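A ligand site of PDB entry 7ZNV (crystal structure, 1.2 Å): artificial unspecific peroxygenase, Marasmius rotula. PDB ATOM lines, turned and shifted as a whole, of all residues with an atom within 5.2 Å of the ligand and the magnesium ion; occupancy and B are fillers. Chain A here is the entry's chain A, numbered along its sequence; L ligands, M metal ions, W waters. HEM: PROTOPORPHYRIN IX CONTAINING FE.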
ATOM      1  N   PRO A  23      24.989 -13.375 -20.755  1.00  0.00           N
ATOM      2  CA  PRO A  23      24.382 -12.081 -20.999  1.00  0.00           C
ATOM      3  C   PRO A  23      24.235 -11.209 -19.748  1.00  0.00           C
ATOM      4  O   PRO A  23      23.599 -10.179 -19.795  1.00  0.00           O
ATOM      5  CB  PRO A  23      23.020 -12.426 -21.605  1.00  0.00           C
ATOM      6  CG  PRO A  23      23.042 -13.916 -21.884  1.00  0.00           C
ATOM      7  CD  PRO A  23      23.999 -14.459 -20.840  1.00  0.00           C
ATOM      8  N   CYS A  24      24.784 -11.686 -18.626  1.00  0.00           N
ATOM      9  CA  CYS A  24      24.559 -11.094 -17.296  1.00  0.00           C
ATOM     10  C   CYS A  24      25.774 -10.348 -16.822  1.00  0.00           C
ATOM     11  O   CYS A  24      26.835 -10.947 -16.596  1.00  0.00           O
ATOM     12  CB  CYS A  24      24.262 -12.182 -16.287  1.00  0.00           C
ATOM     13  SG  CYS A  24      24.043 -11.524 -14.611  1.00  0.00           S
ATOM     14  N   PRO A  25      25.731  -9.018 -16.694  1.00  0.00           N
ATOM     15  CA  PRO A  25      26.881  -8.285 -16.156  1.00  0.00           C
ATOM     16  C   PRO A  25      27.182  -8.704 -14.722  1.00  0.00           C
ATOM     17  O   PRO A  25      28.346  -8.607 -14.304  1.00  0.00           O
ATOM     18  CB  PRO A  25      26.454  -6.825 -16.269  1.00  0.00           C
ATOM     19  CG  PRO A  25      24.956  -6.872 -16.143  1.00  0.00           C
ATOM     20  CD  PRO A  25      24.560  -8.139 -16.903  1.00  0.00           C
ATOM     21  N   GLY A  26      26.170  -9.130 -13.965  1.00  0.00           N
ATOM     22  CA  GLY A  26      26.394  -9.538 -12.580  1.00  0.00           C
ATOM     23  C   GLY A  26      27.315 -10.728 -12.510  1.00  0.00           C
ATOM     24  O   GLY A  26      28.357 -10.719 -11.811  1.00  0.00           O
ATOM     25  N   LEU A  27      26.969 -11.805 -13.171  1.00  0.00           N
ATOM     26  CA  LEU A  27      27.796 -13.010 -13.163  1.00  0.00           C
ATOM     27  C   LEU A  27      29.101 -12.779 -13.873  1.00  0.00           C
ATOM     28  O   LEU A  27      30.134 -13.315 -13.461  1.00  0.00           O
ATOM     29  CB  LEU A  27      27.042 -14.197 -13.747  1.00  0.00           C
ATOM     30  CG  LEU A  27      25.716 -14.574 -13.089  1.00  0.00           C
ATOM     31  CD1 LEU A  27      25.219 -15.857 -13.746  1.00  0.00           C
ATOM     32  CD2 LEU A  27      25.887 -14.745 -11.583  1.00  0.00           C
ATOM     33  N   LEU A  30      31.583 -11.086 -11.643  1.00  0.00           N
ATOM     34  CA  LEU A  30      32.049 -12.035 -10.646  1.00  0.00           C
ATOM     35  C   LEU A  30      33.100 -12.926 -11.277  1.00  0.00           C
ATOM     36  O   LEU A  30      34.138 -13.223 -10.606  1.00  0.00           O
ATOM     37  CB  LEU A  30      30.914 -12.851 -10.053  1.00  0.00           C
ATOM     38  CG  LEU A  30      29.942 -12.064  -9.226  1.00  0.00           C
ATOM     39  CD1 LEU A  30      28.717 -12.914  -8.845  1.00  0.00           C
ATOM     40  CD2 LEU A  30      30.546 -11.451  -7.961  1.00  0.00           C
ATOM     41  N   ILE A  48      27.400 -20.151  -7.362  1.00  0.00           N
ATOM     42  CA  ILE A  48      26.703 -18.883  -7.641  1.00  0.00           C
ATOM     43  C   ILE A  48      26.368 -18.209  -6.314  1.00  0.00           C
ATOM     44  O   ILE A  48      26.558 -16.994  -6.164  1.00  0.00           O
ATOM     45  CB  ILE A  48      25.398 -19.173  -8.414  1.00  0.00           C
ATOM     46  CG1 ILE A  48      25.717 -19.635  -9.834  1.00  0.00           C
ATOM     47  CG2 ILE A  48      24.482 -17.957  -8.342  1.00  0.00           C
ATOM     48  CD1 ILE A  48      26.181 -18.552 -10.754  1.00  0.00           C
ATOM     49  N   GLY A  52      27.923 -14.547  -5.339  1.00  0.00           N
ATOM     50  CA  GLY A  52      27.067 -13.378  -5.172  1.00  0.00           C
ATOM     51  C   GLY A  52      27.206 -12.782  -3.789  1.00  0.00           C
ATOM     52  O   GLY A  52      27.163 -11.561  -3.635  1.00  0.00           O
ATOM     53  N   TYR A  56      29.085  -9.142  -3.844  1.00  0.00           N
ATOM     54  CA  TYR A  56      28.037  -8.110  -3.787  1.00  0.00           C
ATOM     55  C   TYR A  56      27.261  -8.018  -2.508  1.00  0.00           C
ATOM     56  O   TYR A  56      26.462  -7.138  -2.356  1.00  0.00           O
ATOM     57  CB  TYR A  56      27.030  -8.339  -4.935  1.00  0.00           C
ATOM     58  CG  TYR A  56      27.561  -8.402  -6.343  1.00  0.00           C
ATOM     59  CD1 TYR A  56      28.443  -7.447  -6.861  1.00  0.00           C
ATOM     60  CD2 TYR A  56      27.101  -9.371  -7.240  1.00  0.00           C
ATOM     61  CE1 TYR A  56      28.856  -7.487  -8.172  1.00  0.00           C
ATOM     62  CE2 TYR A  56      27.514  -9.422  -8.560  1.00  0.00           C
ATOM     63  CZ  TYR A  56      28.404  -8.490  -9.000  1.00  0.00           C
ATOM     64  OH  TYR A  56      28.874  -8.512 -10.312  1.00  0.00           O
ATOM     65  N   VAL A  58      24.973 -10.159  -1.915  1.00  0.00           N
ATOM     66  CA  VAL A  58      23.620 -10.663  -2.286  1.00  0.00           C
ATOM     67  C   VAL A  58      23.420 -12.005  -1.599  1.00  0.00           C
ATOM     68  O   VAL A  58      24.272 -12.860  -1.609  1.00  0.00           O
ATOM     69  CB  VAL A  58      23.482 -10.705  -3.815  1.00  0.00           C
ATOM     70  CG1 VAL A  58      22.169 -11.392  -4.202  1.00  0.00           C
ATOM     71  CG2 VAL A  58      23.564  -9.328  -4.418  1.00  0.00           C
ATOM     72  N   LEU A  63      19.380 -15.796  -5.503  1.00  0.00           N
ATOM     73  CA  LEU A  63      20.390 -16.445  -6.291  1.00  0.00           C
ATOM     74  C   LEU A  63      20.052 -17.915  -6.525  1.00  0.00           C
ATOM     75  O   LEU A  63      20.360 -18.423  -7.567  1.00  0.00           O
ATOM     76  CB  LEU A  63      21.714 -16.310  -5.583  1.00  0.00           C
ATOM     77  CG  LEU A  63      22.239 -14.894  -5.420  1.00  0.00           C
ATOM     78  CD1 LEU A  63      23.568 -14.910  -4.617  1.00  0.00           C
ATOM     79  CD2 LEU A  63      22.441 -14.226  -6.775  1.00  0.00           C
ATOM     80  N   ALA A  66      17.302 -18.315  -9.340  1.00  0.00           N
ATOM     81  CA  ALA A  66      17.899 -17.987 -10.634  1.00  0.00           C
ATOM     82  C   ALA A  66      18.848 -19.079 -11.105  1.00  0.00           C
ATOM     83  O   ALA A  66      18.853 -19.433 -12.255  1.00  0.00           O
ATOM     84  CB  ALA A  66      18.579 -16.645 -10.584  1.00  0.00           C
ATOM     85  N   ALA A  67      19.682 -19.571 -10.175  1.00  0.00           N
ATOM     86  CA  ALA A  67      20.635 -20.594 -10.537  1.00  0.00           C
ATOM     87  C   ALA A  67      19.963 -21.930 -10.900  1.00  0.00           C
ATOM     88  O   ALA A  67      20.405 -22.603 -11.807  1.00  0.00           O
ATOM     89  CB  ALA A  67      21.654 -20.811  -9.444  1.00  0.00           C
ATOM     90  N   GLY A  70      18.747 -21.406 -14.243  1.00  0.00           N
ATOM     91  CA  GLY A  70      19.888 -21.415 -15.127  1.00  0.00           C
ATOM     92  C   GLY A  70      20.347 -22.819 -15.464  1.00  0.00           C
ATOM     93  O   GLY A  70      20.830 -23.047 -16.584  1.00  0.00           O
ATOM     94  N   PHE A  80      26.252 -25.411 -15.048  1.00  0.00           N
ATOM     95  CA  PHE A  80      26.164 -24.697 -16.310  1.00  0.00           C
ATOM     96  C   PHE A  80      27.450 -23.957 -16.556  1.00  0.00           C
ATOM     97  O   PHE A  80      28.261 -23.748 -15.640  1.00  0.00           O
ATOM     98  CB  PHE A  80      24.956 -23.752 -16.384  1.00  0.00           C
ATOM     99  CG  PHE A  80      24.818 -22.725 -15.290  1.00  0.00           C
ATOM    100  CD1 PHE A  80      25.660 -21.632 -15.240  1.00  0.00           C
ATOM    101  CD2 PHE A  80      23.795 -22.789 -14.368  1.00  0.00           C
ATOM    102  CE1 PHE A  80      25.521 -20.685 -14.229  1.00  0.00           C
ATOM    103  CE2 PHE A  80      23.640 -21.847 -13.374  1.00  0.00           C
ATOM    104  CZ  PHE A  80      24.527 -20.805 -13.291  1.00  0.00           C
ATOM    105  N   LEU A  85      23.776 -19.739 -20.428  1.00  0.00           N
ATOM    106  CA  LEU A  85      22.713 -18.848 -19.949  1.00  0.00           C
ATOM    107  C   LEU A  85      22.198 -17.935 -21.039  1.00  0.00           C
ATOM    108  O   LEU A  85      21.174 -17.258 -20.794  1.00  0.00           O
ATOM    109  CB  LEU A  85      23.236 -18.017 -18.787  1.00  0.00           C
ATOM    110  CG  LEU A  85      23.675 -18.779 -17.533  1.00  0.00           C
ATOM    111  CD1 LEU A  85      24.250 -17.813 -16.515  1.00  0.00           C
ATOM    112  CD2 LEU A  85      22.544 -19.586 -16.940  1.00  0.00           C
ATOM    113  N   ILE A  91      15.924 -17.631 -19.115  1.00  0.00           N
ATOM    114  CA  ILE A  91      15.997 -16.331 -18.409  1.00  0.00           C
ATOM    115  C   ILE A  91      16.155 -15.248 -19.480  1.00  0.00           C
ATOM    116  O   ILE A  91      15.466 -14.245 -19.409  1.00  0.00           O
ATOM    117  CB  ILE A  91      17.183 -16.287 -17.415  1.00  0.00           C
ATOM    118  CG1 ILE A  91      17.005 -17.325 -16.296  1.00  0.00           C
ATOM    119  CG2 ILE A  91      17.362 -14.887 -16.865  1.00  0.00           C
ATOM    120  CD1 ILE A  91      18.239 -17.540 -15.454  1.00  0.00           C
ATOM    121  N   GLU A  92      17.099 -15.456 -20.405  1.00  0.00           N
ATOM    122  CA  GLU A  92      17.384 -14.441 -21.447  1.00  0.00           C
ATOM    123  C   GLU A  92      16.085 -14.016 -22.145  1.00  0.00           C
ATOM    124  O   GLU A  92      15.270 -14.861 -22.536  1.00  0.00           O
ATOM    125  CB  GLU A  92      18.479 -14.936 -22.379  1.00  0.00           C
ATOM    126  CG  GLU A  92      19.058 -13.825 -23.220  1.00  0.00           C
ATOM    127  CD  GLU A  92      18.203 -13.332 -24.351  1.00  0.00           C
ATOM    128  OE1 GLU A  92      17.608 -14.200 -25.041  1.00  0.00           O
ATOM    129  OE2 GLU A  92      18.090 -12.116 -24.576  1.00  0.00           O
ATOM    130  N   HIS A  93      15.968 -12.719 -22.301  1.00  0.00           N
ATOM    131  CA  HIS A  93      14.714 -12.122 -22.818  1.00  0.00           C
ATOM    132  C   HIS A  93      15.016 -10.910 -23.697  1.00  0.00           C
ATOM    133  O   HIS A  93      16.119 -10.351 -23.668  1.00  0.00           O
ATOM    134  CB  HIS A  93      13.860 -11.648 -21.635  1.00  0.00           C
ATOM    135  CG  HIS A  93      14.623 -10.758 -20.704  1.00  0.00           C
ATOM    136  ND1 HIS A  93      14.930  -9.438 -21.010  1.00  0.00           N
ATOM    137  CD2 HIS A  93      15.205 -11.006 -19.510  1.00  0.00           C
ATOM    138  CE1 HIS A  93      15.635  -8.916 -20.038  1.00  0.00           C
ATOM    139  NE2 HIS A  93      15.816  -9.849 -19.108  1.00  0.00           N
ATOM    140  N   ASP A  94      14.018 -10.558 -24.487  1.00  0.00           N
ATOM    141  CA  ASP A  94      14.038  -9.327 -25.286  1.00  0.00           C
ATOM    142  C   ASP A  94      14.026  -8.091 -24.411  1.00  0.00           C
ATOM    143  O   ASP A  94      13.694  -8.169 -23.204  1.00  0.00           O
ATOM    144  CB  ASP A  94      12.823  -9.366 -26.204  1.00  0.00           C
ATOM    145  CG  ASP A  94      12.799 -10.532 -27.135  1.00  0.00           C
ATOM    146  OD1 ASP A  94      13.863 -10.992 -27.505  1.00  0.00           O
ATOM    147  OD2 ASP A  94      11.671 -10.972 -27.486  1.00  0.00           O
ATOM    148  N   SER A  96      16.501  -6.212 -23.402  1.00  0.00           N
ATOM    149  CA  SER A  96      17.642  -6.085 -22.483  1.00  0.00           C
ATOM    150  C   SER A  96      18.158  -4.671 -22.480  1.00  0.00           C
ATOM    151  O   SER A  96      17.965  -3.898 -23.422  1.00  0.00           O
ATOM    152  CB  SER A  96      18.722  -7.055 -22.833  1.00  0.00           C
ATOM    153  OG  SER A  96      18.296  -8.402 -22.620  1.00  0.00           O
ATOM    154  N   LEU A  97      18.888  -4.321 -21.421  1.00  0.00           N
ATOM    155  CA  LEU A  97      19.503  -3.010 -21.236  1.00  0.00           C
ATOM    156  C   LEU A  97      20.746  -2.811 -22.056  1.00  0.00           C
ATOM    157  O   LEU A  97      21.082  -1.646 -22.335  1.00  0.00           O
ATOM    158  CB  LEU A  97      19.919  -2.876 -19.760  1.00  0.00           C
ATOM    159  CG  LEU A  97      18.778  -2.983 -18.769  1.00  0.00           C
ATOM    160  CD1 LEU A  97      19.369  -3.171 -17.371  1.00  0.00           C
ATOM    161  CD2 LEU A  97      17.861  -1.803 -18.767  1.00  0.00           C
ATOM    162  N   SER A  98      21.421  -3.865 -22.447  1.00  0.00           N
ATOM    163  CA  SER A  98      22.755  -3.751 -23.014  1.00  0.00           C
ATOM    164  C   SER A  98      23.066  -4.777 -24.086  1.00  0.00           C
ATOM    165  O   SER A  98      24.203  -4.836 -24.565  1.00  0.00           O
ATOM    166  CB  SER A  98      23.815  -3.780 -21.960  1.00  0.00           C
ATOM    167  OG  SER A  98      23.945  -5.032 -21.335  1.00  0.00           O
ATOM    168  N   ARG A  99      22.100  -5.629 -24.409  1.00  0.00           N
ATOM    169  CA  ARG A  99      22.215  -6.675 -25.430  1.00  0.00           C
ATOM    170  C   ARG A  99      21.106  -6.469 -26.438  1.00  0.00           C
ATOM    171  O   ARG A  99      20.075  -5.950 -26.124  1.00  0.00           O
ATOM    172  CB  ARG A  99      22.104  -8.071 -24.812  1.00  0.00           C
ATOM    173  CG  ARG A  99      23.366  -8.705 -24.295  1.00  0.00           C
ATOM    174  CD  ARG A  99      24.043  -7.944 -23.157  1.00  0.00           C
ATOM    175  NE  ARG A  99      25.162  -8.680 -22.680  1.00  0.00           N
ATOM    176  CZ  ARG A  99      26.047  -8.252 -21.772  1.00  0.00           C
ATOM    177  NH1 ARG A  99      25.923  -7.058 -21.276  1.00  0.00           N
ATOM    178  NH2 ARG A  99      27.059  -9.022 -21.436  1.00  0.00           N
ATOM    179  N   GLU A 100      21.327  -6.978 -27.654  1.00  0.00           N
ATOM    180  CA  GLU A 100      20.267  -7.015 -28.693  1.00  0.00           C
ATOM    181  C   GLU A 100      19.335  -8.177 -28.440  1.00  0.00           C
ATOM    182  O   GLU A 100      19.682  -9.163 -27.804  1.00  0.00           O
ATOM    183  CB  GLU A 100      20.949  -7.155 -30.058  1.00  0.00           C
ATOM    184  CG  GLU A 100      21.885  -6.021 -30.404  1.00  0.00           C
ATOM    185  CD  GLU A 100      22.690  -6.191 -31.684  1.00  0.00           C
ATOM    186  OE1 GLU A 100      23.104  -7.311 -32.009  1.00  0.00           O
ATOM    187  OE2 GLU A 100      22.976  -5.137 -32.307  1.00  0.00           O
ATOM    188  N   ASN A 107      22.384 -11.671 -28.636  1.00  0.00           N
ATOM    189  CA  ASN A 107      21.713 -11.614 -27.312  1.00  0.00           C
ATOM    190  C   ASN A 107      22.667 -11.820 -26.138  1.00  0.00           C
ATOM    191  O   ASN A 107      22.196 -11.915 -25.001  1.00  0.00           O
ATOM    192  CB  ASN A 107      20.533 -12.571 -27.201  1.00  0.00           C
ATOM    193  CG  ASN A 107      20.939 -13.996 -27.004  1.00  0.00           C
ATOM    194  OD1 ASN A 107      22.122 -14.360 -27.208  1.00  0.00           O
ATOM    195  ND2 ASN A 107      20.057 -14.867 -26.575  1.00  0.00           N
ATOM    196  N   GLU A 164      16.268  -7.155 -12.656  1.00  0.00           N
ATOM    197  CA  GLU A 164      17.627  -6.864 -13.176  1.00  0.00           C
ATOM    198  C   GLU A 164      17.960  -5.383 -12.991  1.00  0.00           C
ATOM    199  O   GLU A 164      19.084  -5.072 -12.621  1.00  0.00           O
ATOM    200  CB  GLU A 164      17.712  -7.322 -14.635  1.00  0.00           C
ATOM    201  CG  GLU A 164      17.816  -8.829 -14.681  1.00  0.00           C
ATOM    202  CD  GLU A 164      17.510  -9.544 -15.986  1.00  0.00           C
ATOM    203  OE1 GLU A 164      17.002  -8.891 -16.896  1.00  0.00           O
ATOM    204  OE2 GLU A 164      17.786 -10.767 -16.057  1.00  0.00           O
ATOM    205  N   SER A 165      16.981  -4.524 -13.210  1.00  0.00           N
ATOM    206  CA  SER A 165      17.240  -3.076 -13.029  1.00  0.00           C
ATOM    207  C   SER A 165      17.424  -2.792 -11.527  1.00  0.00           C
ATOM    208  O   SER A 165      18.316  -2.038 -11.169  1.00  0.00           O
ATOM    209  CB  SER A 165      16.154  -2.252 -13.693  1.00  0.00           C
ATOM    210  OG  SER A 165      16.371  -2.218 -15.100  1.00  0.00           O
ATOM    211  N   PHE A 167      18.720  -4.841  -9.510  1.00  0.00           N
ATOM    212  CA  PHE A 167      20.075  -5.385  -9.264  1.00  0.00           C
ATOM    213  C   PHE A 167      21.162  -4.351  -9.606  1.00  0.00           C
ATOM    214  O   PHE A 167      22.066  -4.188  -8.805  1.00  0.00           O
ATOM    215  CB  PHE A 167      20.284  -6.694 -10.020  1.00  0.00           C
ATOM    216  CG  PHE A 167      20.149  -7.950  -9.189  1.00  0.00           C
ATOM    217  CD1 PHE A 167      20.781  -8.076  -7.968  1.00  0.00           C
ATOM    218  CD2 PHE A 167      19.408  -9.017  -9.661  1.00  0.00           C
ATOM    219  CE1 PHE A 167      20.659  -9.242  -7.221  1.00  0.00           C
ATOM    220  CE2 PHE A 167      19.294 -10.177  -8.922  1.00  0.00           C
ATOM    221  CZ  PHE A 167      19.921 -10.290  -7.707  1.00  0.00           C
ATOM    222  N   TYR A 168      21.111  -3.727 -10.785  1.00  0.00           N
ATOM    223  CA  TYR A 168      22.250  -2.815 -11.118  1.00  0.00           C
ATOM    224  C   TYR A 168      22.213  -1.631 -10.151  1.00  0.00           C
ATOM    225  O   TYR A 168      23.268  -1.177  -9.724  1.00  0.00           O
ATOM    226  CB  TYR A 168      22.329  -2.416 -12.610  1.00  0.00           C
ATOM    227  CG  TYR A 168      21.349  -1.393 -13.139  1.00  0.00           C
ATOM    228  CD1 TYR A 168      21.458  -0.047 -12.810  1.00  0.00           C
ATOM    229  CD2 TYR A 168      20.359  -1.762 -14.031  1.00  0.00           C
ATOM    230  CE1 TYR A 168      20.576   0.888 -13.318  1.00  0.00           C
ATOM    231  CE2 TYR A 168      19.465  -0.832 -14.543  1.00  0.00           C
ATOM    232  CZ  TYR A 168      19.577   0.502 -14.187  1.00  0.00           C
ATOM    233  OH  TYR A 168      18.708   1.433 -14.677  1.00  0.00           O
ATOM    234  N   VAL A 171      23.473  -3.229  -6.549  1.00  0.00           N
ATOM    235  CA  VAL A 171      24.853  -3.721  -6.372  1.00  0.00           C
ATOM    236  C   VAL A 171      25.846  -2.622  -6.694  1.00  0.00           C
ATOM    237  O   VAL A 171      26.909  -2.623  -6.017  1.00  0.00           O
ATOM    238  CB  VAL A 171      25.196  -5.033  -7.088  1.00  0.00           C
ATOM    239  CG1 VAL A 171      24.094  -6.027  -6.752  1.00  0.00           C
ATOM    240  CG2 VAL A 171      25.364  -4.949  -8.609  1.00  0.00           C
ATOM    241  N   PHE A 188      30.470  -1.055 -14.741  1.00  0.00           N
ATOM    242  CA  PHE A 188      29.901  -2.393 -14.527  1.00  0.00           C
ATOM    243  C   PHE A 188      29.473  -3.010 -15.867  1.00  0.00           C
ATOM    244  O   PHE A 188      29.813  -4.162 -16.173  1.00  0.00           O
ATOM    245  CB  PHE A 188      28.773  -2.274 -13.517  1.00  0.00           C
ATOM    246  CG  PHE A 188      28.005  -3.529 -13.190  1.00  0.00           C
ATOM    247  CD1 PHE A 188      28.609  -4.564 -12.525  1.00  0.00           C
ATOM    248  CD2 PHE A 188      26.644  -3.597 -13.457  1.00  0.00           C
ATOM    249  CE1 PHE A 188      27.837  -5.684 -12.176  1.00  0.00           C
ATOM    250  CE2 PHE A 188      25.893  -4.705 -13.113  1.00  0.00           C
ATOM    251  CZ  PHE A 188      26.517  -5.706 -12.459  1.00  0.00           C
ATOM    252  N   PHE A 189      28.676  -2.298 -16.631  1.00  0.00           N
ATOM    253  CA  PHE A 189      28.170  -2.834 -17.903  1.00  0.00           C
ATOM    254  C   PHE A 189      29.274  -2.899 -18.959  1.00  0.00           C
ATOM    255  O   PHE A 189      29.422  -3.904 -19.660  1.00  0.00           O
ATOM    256  CB  PHE A 189      26.998  -2.031 -18.409  1.00  0.00           C
ATOM    257  CG  PHE A 189      25.685  -2.371 -17.789  1.00  0.00           C
ATOM    258  CD1 PHE A 189      24.865  -3.332 -18.390  1.00  0.00           C
ATOM    259  CD2 PHE A 189      25.215  -1.743 -16.671  1.00  0.00           C
ATOM    260  CE1 PHE A 189      23.621  -3.609 -17.889  1.00  0.00           C
ATOM    261  CE2 PHE A 189      23.970  -2.073 -16.122  1.00  0.00           C
ATOM    262  CZ  PHE A 189      23.184  -3.028 -16.733  1.00  0.00           C
HETATM  263  CHA HEM L   1      20.760 -10.208 -16.963  1.00  0.00           C
HETATM  264  CHB HEM L   1      22.496  -8.401 -12.838  1.00  0.00           C
HETATM  265  CHC HEM L   1      22.657 -12.898 -10.988  1.00  0.00           C
HETATM  266  CHD HEM L   1      21.379 -14.698 -15.289  1.00  0.00           C
HETATM  267  C1A HEM L   1      21.127  -9.358 -15.967  1.00  0.00           C
HETATM  268  C2A HEM L   1      21.031  -7.947 -16.074  1.00  0.00           C
HETATM  269  C3A HEM L   1      21.508  -7.425 -14.914  1.00  0.00           C
HETATM  270  C4A HEM L   1      21.905  -8.514 -14.094  1.00  0.00           C
HETATM  271  CMA HEM L   1      21.621  -5.959 -14.567  1.00  0.00           C
HETATM  272  CAA HEM L   1      20.478  -7.186 -17.256  1.00  0.00           C
HETATM  273  CBA HEM L   1      21.468  -7.072 -18.409  1.00  0.00           C
HETATM  274  CGA HEM L   1      20.837  -6.364 -19.580  1.00  0.00           C
HETATM  275  O1A HEM L   1      21.542  -5.937 -20.489  1.00  0.00           O
HETATM  276  O2A HEM L   1      19.600  -6.194 -19.624  1.00  0.00           O
HETATM  277  C1B HEM L   1      22.717  -9.498 -11.996  1.00  0.00           C
HETATM  278  C2B HEM L   1      23.234  -9.361 -10.677  1.00  0.00           C
HETATM  279  C3B HEM L   1      23.295 -10.607 -10.142  1.00  0.00           C
HETATM  280  C4B HEM L   1      22.785 -11.526 -11.175  1.00  0.00           C
HETATM  281  CMB HEM L   1      23.658  -8.077  -9.998  1.00  0.00           C
HETATM  282  CAB HEM L   1      23.751 -10.966  -8.787  1.00  0.00           C
HETATM  283  CBB HEM L   1      24.636 -11.949  -8.604  1.00  0.00           C
HETATM  284  C1C HEM L   1      22.254 -13.787 -11.969  1.00  0.00           C
HETATM  285  C2C HEM L   1      22.060 -15.163 -11.800  1.00  0.00           C
HETATM  286  C3C HEM L   1      21.697 -15.673 -13.023  1.00  0.00           C
HETATM  287  C4C HEM L   1      21.656 -14.583 -13.951  1.00  0.00           C
HETATM  288  CMC HEM L   1      22.226 -15.909 -10.483  1.00  0.00           C
HETATM  289  CAC HEM L   1      21.401 -17.089 -13.354  1.00  0.00           C
HETATM  290  CBC HEM L   1      22.164 -18.060 -12.880  1.00  0.00           C
HETATM  291  C1D HEM L   1      21.134 -13.577 -16.092  1.00  0.00           C
HETATM  292  C2D HEM L   1      20.701 -13.713 -17.495  1.00  0.00           C
HETATM  293  C3D HEM L   1      20.522 -12.466 -17.950  1.00  0.00           C
HETATM  294  C4D HEM L   1      20.857 -11.584 -16.830  1.00  0.00           C
HETATM  295  CMD HEM L   1      20.502 -15.003 -18.273  1.00  0.00           C
HETATM  296  CAD HEM L   1      20.083 -12.048 -19.334  1.00  0.00           C
HETATM  297  CBD HEM L   1      18.659 -11.496 -19.320  1.00  0.00           C
HETATM  298  CGD HEM L   1      18.506 -10.575 -20.505  1.00  0.00           C
HETATM  299  O1D HEM L   1      18.050 -10.993 -21.580  1.00  0.00           O
HETATM  300  O2D HEM L   1      18.859  -9.390 -20.386  1.00  0.00           O
HETATM  301  NA  HEM L   1      21.652  -9.687 -14.734  1.00  0.00           N
HETATM  302  NB  HEM L   1      22.461 -10.786 -12.237  1.00  0.00           N
HETATM  303  NC  HEM L   1      21.994 -13.457 -13.261  1.00  0.00           N
HETATM  304  ND  HEM L   1      21.214 -12.283 -15.730  1.00  0.00           N
HETATM  305 FE   HEM L   1      21.770 -11.545 -14.045  1.00  0.00          FE
HETATM  306 MG    MG M   1      18.238 -10.312 -23.576  1.00  0.00          MG
HETATM  307  O   HOH W   1      21.588  -9.287 -21.462  1.00  0.00           O
HETATM  308  O   HOH W   2      17.186  -6.431 -18.360  1.00  0.00           O
HETATM  309  O   HOH W   3      19.832 -11.533 -13.549  1.00  0.00           O
HETATM  310  O   HOH W   4      20.287 -10.537 -23.474  1.00  0.00           O
HETATM  311  O   HOH W   5      18.296  -9.335 -25.422  1.00  0.00           O
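Water W2 lies within hydrogen-bond range of an oxygen (O2A) of the ligand (2.7 Å) and the side-chain carboxylate of Glu 164 (2.9 Å).
Water W1 bridges O of Pro 23 (2.8 Å) and O2D of the ligand (2.9 Å).
OH of Tyr 56 sits at hydrogen-bond distance from O of Gly 26 (2.7 Å).
The side-chain carboxylate (OE1) of Glu 92 lies within hydrogen-bond range of the side-chain amide nitrogen (ND2) of Asn 107 (3.0 Å).
The side-chain hydroxyl (OG) of Ser 98 is in hydrogen-bond range of the guanidinium group (NH1) of Arg 99 (2.8 Å).
N of Gly 26 lies close to SG of Cys 24.
The side-chain carboxylate of Glu 164 is in hydrogen-bond range of a ring nitrogen (NE2) of His 93 (2.7 Å).
The backbone NH (N) of Leu 27 lies close to the side-chain sulfur (SG) of Cys 24 (3.3 Å).
The magnesium ion is bound by water W4 (2.1 Å), OE2 of Glu 92 (2.1 Å), water W5 (2.1 Å), O1D of the ligand (2.1 Å), O of His 93 (2.1 Å) and OG of Ser 96 (2.1 Å).
Within 4 Å of the magnesium ion: Glu 92, His 93 and Ser 96.
An oxygen (O2A) of the ligand is in hydrogen-bond range of the backbone NH (N) of Leu 97 (2.7 Å).
An oxygen (O1A) of the ligand sits at hydrogen-bond distance from the side-chain hydroxyl of Ser 98 (2.7 Å).
NE2 of His 93 lies close to O2D of the ligand, 3.3 Å away.
The backbone NH (N) of Ser 98 lies within hydrogen-bond range of an oxygen (O1A) of the ligand (2.9 Å).
The backbone NH of His 93 sits close to an oxygen (O1D) of the ligand (2.8 Å).
The side-chain sulfur (SG) of Cys 24 binds an iron atom (FE) of the ligand (2.3 Å).
Pro 23 touches the ligand (CB to CAD, 3.7 Å).
CD of Pro 25 touches CBA of the ligand, 3.6 Å away.
CA of Gly 26 touches C2B of the ligand (3.7 Å).
Leu 27 touches the ligand (CD1 to C3C, 3.6 Å).
Ile 48 touches the ligand (CG2 to CMC, 3.7 Å).
CD2 of Tyr 56 touches CBB of the ligand, 3.8 Å away.
Leu 63 touches the ligand (CD2 to CBB, 3.7 Å).
Ala 66 touches the ligand.
Ala 67 touches the ligand.
Phe 80 touches the ligand (CZ to CBC, 3.6 Å).
Leu 85 touches the ligand (O to CMD, 3.4 Å).
Ile 91 touches the ligand.
Arg 99 touches the ligand (N to O1A, 3.97 Å).
OE2 of Glu 164 touches CHA of the ligand (3.2 Å).
Phe 167 touches the ligand.
CG2 of Val 171 touches CMB of the ligand, at 3.8 Å.
Phe 189 touches the ligand.
Hydrophobic or aromatic side chains that line the ligand: Pro 23, Pro 25, Leu 27, Ile 48, Tyr 56, Leu 63, Ala 66, Phe 80, Ile 91, His 93, Leu 97, Phe 167, Val 171 and Phe 189.
23 residues have an atom within 4 Å of the ligand: Pro 23, Cys 24, Pro 25, Gly 26, Leu 27, Ile 48, Tyr 56, Leu 63, Ala 66, Ala 67, Phe 80, Leu 85, Ile 91, Glu 92, His 93, Ser 96, Leu 97, Ser 98, Arg 99, Glu 164, Phe 167, Val 171 and Phe 189.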
